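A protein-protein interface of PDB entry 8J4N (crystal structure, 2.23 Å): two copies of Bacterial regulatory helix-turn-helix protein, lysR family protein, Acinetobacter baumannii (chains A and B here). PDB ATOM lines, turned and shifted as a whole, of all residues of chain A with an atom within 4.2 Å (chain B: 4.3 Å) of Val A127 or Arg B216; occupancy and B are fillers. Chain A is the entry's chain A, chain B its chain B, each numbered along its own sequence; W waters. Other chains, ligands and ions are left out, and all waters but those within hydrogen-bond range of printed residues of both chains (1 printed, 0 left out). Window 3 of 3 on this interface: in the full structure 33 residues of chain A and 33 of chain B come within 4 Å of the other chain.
Among the printed residues, merely in contact across the chains: Ile A126 with Asp B218, Val A127 with Arg B216 and Val A127 with Asp B218.
Of the 9 printed residues of chain A, 4 touch a printed residue of chain B. Hydrophobic or aromatic side chains of chain A that line the printed part of chain B: Val A127. Along chain A the printed residues that touch a printed residue of chain B span positions 125 to 128. Printed residues of chain B that touch a printed residue of chain A: Arg B216, Thr B217 and Asp B218. Among the printed residues, 7 pairs touch across the chains.
Water W1 lies within hydrogen-bond range of OD1 of Asp B218 (2.9 Å), O of Ile A126 (3.1 Å) and OG1 of Thr B217 (3.4 Å).
N of Ile A97 is in hydrogen-bond range of O of Asn A125. The backbone carbonyl oxygen of Val A127 is in hydrogen-bond range of the backbone NH of Val A99. The backbone carbonyl oxygen of Ile A97 sits at hydrogen-bond distance from the backbone NH of Val A127, at 2.9 Å. The guanidinium group of Arg B216 is in hydrogen-bond range of the backbone carbonyl oxygen of Ala B198 (3.0 Å). N of Thr B217 sits at hydrogen-bond distance from O of Val B196 (2.7 Å). O of Thr B217 sits at hydrogen-bond distance from N of Ala B198 (2.9 Å).
The backbone NH of Arg B216 lies within hydrogen-bond range of the side-chain amide oxygen of Asn A125, at 3.0 Å. N of Ile A126 sits at hydrogen-bond distance from O of Arg B216, at 3.3 Å. N of Ser A128 sits at hydrogen-bond distance from OD2 of Asp B218 (2.9 Å). O of Ile A126 is in hydrogen-bond range of OG1 of Thr B217 (2.9 Å).
Val A98 touches none of the printed residues of chain B. Of the printed residues of chain B, Asn A125 touches Arg B216. Of chain B, only Arg B216 (3.6 Å) and Asp B218 (3.7 Å) come within 4 Å of Val A127. Printed residues of chain B within 4 Å of Ser A128: Asp B218 (2.9 Å). Ser B199 touches none of the printed residues of chain A. Arg B216 touches three residues of chain A. Printed residues of chain A within 4 Å of Asp B218: Ile A126, Val A127 and Ser A128. The nearest printed residue of chain B that does not touch Val A127 is Thr B217 (5.1 Å). The nearest printed residue of chain A that does not touch Arg B216 is Thr A96 (5.4 Å).
No position is printed for both chains.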
ATOM      1  N   THR A  96      -4.962 -21.301  -2.217  1.00  0.00           N
ATOM      2  CA  THR A  96      -5.200 -20.142  -1.366  1.00  0.00           C
ATOM      3  C   THR A  96      -6.120 -19.164  -2.081  1.00  0.00           C
ATOM      4  O   THR A  96      -5.835 -18.740  -3.208  1.00  0.00           O
ATOM      5  CB  THR A  96      -3.891 -19.446  -0.981  1.00  0.00           C
ATOM      6  OG1 THR A  96      -3.081 -20.344  -0.213  1.00  0.00           O
ATOM      7  CG2 THR A  96      -4.175 -18.193  -0.148  1.00  0.00           C
ATOM      8  N   ILE A  97      -7.211 -18.803  -1.411  1.00  0.00           N
ATOM      9  CA  ILE A  97      -8.212 -17.881  -1.926  1.00  0.00           C
ATOM     10  C   ILE A  97      -8.247 -16.675  -0.999  1.00  0.00           C
ATOM     11  O   ILE A  97      -8.388 -16.834   0.218  1.00  0.00           O
ATOM     12  CB  ILE A  97      -9.595 -18.550  -1.996  1.00  0.00           C
ATOM     13  CG1 ILE A  97      -9.532 -19.817  -2.852  1.00  0.00           C
ATOM     14  CG2 ILE A  97     -10.638 -17.574  -2.519  1.00  0.00           C
ATOM     15  CD1 ILE A  97     -10.835 -20.583  -2.902  1.00  0.00           C
ATOM     16  N   VAL A  98      -8.112 -15.478  -1.567  1.00  0.00           N
ATOM     17  CA  VAL A  98      -8.179 -14.250  -0.781  1.00  0.00           C
ATOM     18  C   VAL A  98      -9.542 -13.603  -0.996  1.00  0.00           C
ATOM     19  O   VAL A  98      -9.915 -13.268  -2.125  1.00  0.00           O
ATOM     20  CB  VAL A  98      -7.033 -13.281  -1.123  1.00  0.00           C
ATOM     21  CG1 VAL A  98      -6.952 -13.006  -2.617  1.00  0.00           C
ATOM     22  CG2 VAL A  98      -7.189 -11.978  -0.348  1.00  0.00           C
ATOM     23  N   VAL A  99     -10.296 -13.455   0.087  1.00  0.00           N
ATOM     24  CA  VAL A  99     -11.571 -12.753   0.078  1.00  0.00           C
ATOM     25  C   VAL A  99     -11.310 -11.340   0.572  1.00  0.00           C
ATOM     26  O   VAL A  99     -10.806 -11.153   1.684  1.00  0.00           O
ATOM     27  CB  VAL A  99     -12.606 -13.464   0.963  1.00  0.00           C
ATOM     28  CG1 VAL A  99     -13.946 -12.748   0.888  1.00  0.00           C
ATOM     29  CG2 VAL A  99     -12.738 -14.926   0.565  1.00  0.00           C
ATOM     30  N   ASN A 125      -6.898 -22.779   1.804  1.00  0.00           N
ATOM     31  CA  ASN A 125      -6.661 -21.699   2.751  1.00  0.00           C
ATOM     32  C   ASN A 125      -7.420 -20.453   2.320  1.00  0.00           C
ATOM     33  O   ASN A 125      -7.236 -19.960   1.202  1.00  0.00           O
ATOM     34  CB  ASN A 125      -5.166 -21.400   2.878  1.00  0.00           C
ATOM     35  CG  ASN A 125      -4.347 -22.649   3.149  1.00  0.00           C
ATOM     36  OD1 ASN A 125      -4.610 -23.379   4.106  1.00  0.00           O
ATOM     37  ND2 ASN A 125      -3.346 -22.898   2.314  1.00  0.00           N
ATOM     38  N   ILE A 126      -8.268 -19.948   3.209  1.00  0.00           N
ATOM     39  CA  ILE A 126      -9.076 -18.761   2.959  1.00  0.00           C
ATOM     40  C   ILE A 126      -8.479 -17.623   3.779  1.00  0.00           C
ATOM     41  O   ILE A 126      -8.538 -17.643   5.013  1.00  0.00           O
ATOM     42  CB  ILE A 126     -10.552 -18.989   3.317  1.00  0.00           C
ATOM     43  CG1 ILE A 126     -11.082 -20.251   2.633  1.00  0.00           C
ATOM     44  CG2 ILE A 126     -11.384 -17.779   2.937  1.00  0.00           C
ATOM     45  CD1 ILE A 126     -11.211 -20.114   1.137  1.00  0.00           C
ATOM     46  N   VAL A 127      -7.896 -16.636   3.097  1.00  0.00           N
ATOM     47  CA  VAL A 127      -7.355 -15.452   3.747  1.00  0.00           C
ATOM     48  C   VAL A 127      -8.173 -14.235   3.319  1.00  0.00           C
ATOM     49  O   VAL A 127      -8.972 -14.290   2.384  1.00  0.00           O
ATOM     50  CB  VAL A 127      -5.856 -15.251   3.441  1.00  0.00           C
ATOM     51  CG1 VAL A 127      -5.043 -16.416   3.980  1.00  0.00           C
ATOM     52  CG2 VAL A 127      -5.636 -15.079   1.946  1.00  0.00           C
ATOM     53  N   SER A 128      -7.968 -13.124   4.025  1.00  0.00           N
ATOM     54  CA  SER A 128      -8.648 -11.873   3.734  1.00  0.00           C
ATOM     55  C   SER A 128      -7.631 -10.744   3.688  1.00  0.00           C
ATOM     56  O   SER A 128      -6.589 -10.800   4.347  1.00  0.00           O
ATOM     57  CB  SER A 128      -9.742 -11.567   4.770  1.00  0.00           C
ATOM     58  OG  SER A 128      -9.226 -11.557   6.088  1.00  0.00           O
ATOM     59  N   MET A 137      -1.487 -10.151  -4.233  1.00  0.00           N
ATOM     60  CA  MET A 137      -1.331 -11.562  -3.891  1.00  0.00           C
ATOM     61  C   MET A 137      -1.514 -12.451  -5.113  1.00  0.00           C
ATOM     62  O   MET A 137      -0.819 -13.463  -5.264  1.00  0.00           O
ATOM     63  CB  MET A 137      -2.323 -11.947  -2.796  1.00  0.00           C
ATOM     64  CG  MET A 137      -2.008 -11.340  -1.445  1.00  0.00           C
ATOM     65  SD  MET A 137      -3.223 -11.813  -0.201  1.00  0.00           S
ATOM     66  CE  MET A 137      -2.645 -13.447   0.238  1.00  0.00           C
ATOM     67  N   VAL B 196      -7.719 -24.150  11.182  1.00  0.00           N
ATOM     68  CA  VAL B 196      -6.764 -23.437  12.023  1.00  0.00           C
ATOM     69  C   VAL B 196      -6.793 -21.959  11.656  1.00  0.00           C
ATOM     70  O   VAL B 196      -6.862 -21.609  10.472  1.00  0.00           O
ATOM     71  CB  VAL B 196      -5.349 -24.023  11.879  1.00  0.00           C
ATOM     72  CG1 VAL B 196      -4.383 -23.327  12.818  1.00  0.00           C
ATOM     73  CG2 VAL B 196      -5.372 -25.517  12.143  1.00  0.00           C
ATOM     74  N   ALA B 198      -4.599 -18.657  11.775  1.00  0.00           N
ATOM     75  CA  ALA B 198      -3.226 -18.193  11.941  1.00  0.00           C
ATOM     76  C   ALA B 198      -2.826 -17.386  10.710  1.00  0.00           C
ATOM     77  O   ALA B 198      -3.576 -17.295   9.735  1.00  0.00           O
ATOM     78  CB  ALA B 198      -2.262 -19.361  12.173  1.00  0.00           C
ATOM     79  N   SER B 199      -1.631 -16.799  10.780  1.00  0.00           N
ATOM     80  CA  SER B 199      -1.061 -15.979   9.713  1.00  0.00           C
ATOM     81  C   SER B 199      -1.955 -14.798   9.386  1.00  0.00           C
ATOM     82  O   SER B 199      -1.950 -13.803  10.106  1.00  0.00           O
ATOM     83  CB  SER B 199      -0.811 -16.808   8.449  1.00  0.00           C
ATOM     84  OG  SER B 199       0.485 -17.370   8.465  1.00  0.00           O
ATOM     85  N   LEU B 204       2.791 -21.201  11.505  1.00  0.00           N
ATOM     86  CA  LEU B 204       2.021 -22.174  12.278  1.00  0.00           C
ATOM     87  C   LEU B 204       2.852 -22.800  13.396  1.00  0.00           C
ATOM     88  O   LEU B 204       3.838 -23.497  13.134  1.00  0.00           O
ATOM     89  CB  LEU B 204       1.464 -23.253  11.354  1.00  0.00           C
ATOM     90  CG  LEU B 204       0.132 -22.882  10.708  1.00  0.00           C
ATOM     91  CD1 LEU B 204      -0.139 -23.790   9.538  1.00  0.00           C
ATOM     92  CD2 LEU B 204      -0.992 -22.968  11.723  1.00  0.00           C
ATOM     93  N   TRP B 215      -6.743 -27.041   7.363  1.00  0.00           N
ATOM     94  CA  TRP B 215      -6.860 -25.830   6.568  1.00  0.00           C
ATOM     95  C   TRP B 215      -6.501 -24.630   7.429  1.00  0.00           C
ATOM     96  O   TRP B 215      -6.759 -24.611   8.636  1.00  0.00           O
ATOM     97  CB  TRP B 215      -8.280 -25.649   6.028  1.00  0.00           C
ATOM     98  CG  TRP B 215      -8.693 -26.621   4.982  1.00  0.00           C
ATOM     99  CD1 TRP B 215      -7.952 -27.639   4.459  1.00  0.00           C
ATOM    100  CD2 TRP B 215      -9.964 -26.672   4.332  1.00  0.00           C
ATOM    101  NE1 TRP B 215      -8.685 -28.319   3.518  1.00  0.00           N
ATOM    102  CE2 TRP B 215      -9.926 -27.744   3.422  1.00  0.00           C
ATOM    103  CE3 TRP B 215     -11.132 -25.911   4.432  1.00  0.00           C
ATOM    104  CZ2 TRP B 215     -11.011 -28.075   2.615  1.00  0.00           C
ATOM    105  CZ3 TRP B 215     -12.206 -26.240   3.633  1.00  0.00           C
ATOM    106  CH2 TRP B 215     -12.140 -27.311   2.735  1.00  0.00           C
ATOM    107  N   ARG B 216      -5.915 -23.617   6.801  1.00  0.00           N
ATOM    108  CA  ARG B 216      -5.567 -22.382   7.487  1.00  0.00           C
ATOM    109  C   ARG B 216      -6.470 -21.256   7.007  1.00  0.00           C
ATOM    110  O   ARG B 216      -6.661 -21.077   5.800  1.00  0.00           O
ATOM    111  CB  ARG B 216      -4.103 -22.012   7.258  1.00  0.00           C
ATOM    112  CG  ARG B 216      -3.580 -20.979   8.237  1.00  0.00           C
ATOM    113  CD  ARG B 216      -2.143 -20.623   7.914  1.00  0.00           C
ATOM    114  NE  ARG B 216      -1.970 -20.086   6.567  1.00  0.00           N
ATOM    115  CZ  ARG B 216      -2.531 -18.973   6.108  1.00  0.00           C
ATOM    116  NH1 ARG B 216      -3.300 -18.214   6.871  1.00  0.00           N
ATOM    117  NH2 ARG B 216      -2.299 -18.601   4.851  1.00  0.00           N
ATOM    118  N   THR B 217      -7.034 -20.515   7.955  1.00  0.00           N
ATOM    119  CA  THR B 217      -7.752 -19.277   7.697  1.00  0.00           C
ATOM    120  C   THR B 217      -7.230 -18.230   8.669  1.00  0.00           C
ATOM    121  O   THR B 217      -6.561 -18.555   9.650  1.00  0.00           O
ATOM    122  CB  THR B 217      -9.268 -19.454   7.839  1.00  0.00           C
ATOM    123  OG1 THR B 217      -9.924 -18.244   7.449  1.00  0.00           O
ATOM    124  CG2 THR B 217      -9.627 -19.777   9.271  1.00  0.00           C
ATOM    125  N   ASP B 218      -7.511 -16.958   8.394  1.00  0.00           N
ATOM    126  CA  ASP B 218      -6.904 -15.889   9.177  1.00  0.00           C
ATOM    127  C   ASP B 218      -7.873 -15.200  10.132  1.00  0.00           C
ATOM    128  O   ASP B 218      -7.511 -14.183  10.727  1.00  0.00           O
ATOM    129  CB  ASP B 218      -6.240 -14.855   8.258  1.00  0.00           C
ATOM    130  CG  ASP B 218      -7.226 -14.144   7.352  1.00  0.00           C
ATOM    131  OD1 ASP B 218      -8.422 -14.503   7.340  1.00  0.00           O
ATOM    132  OD2 ASP B 218      -6.794 -13.213   6.647  1.00  0.00           O
HETATM  133  O   HOH W   1     -10.623 -15.457   5.657  1.00  0.00           O
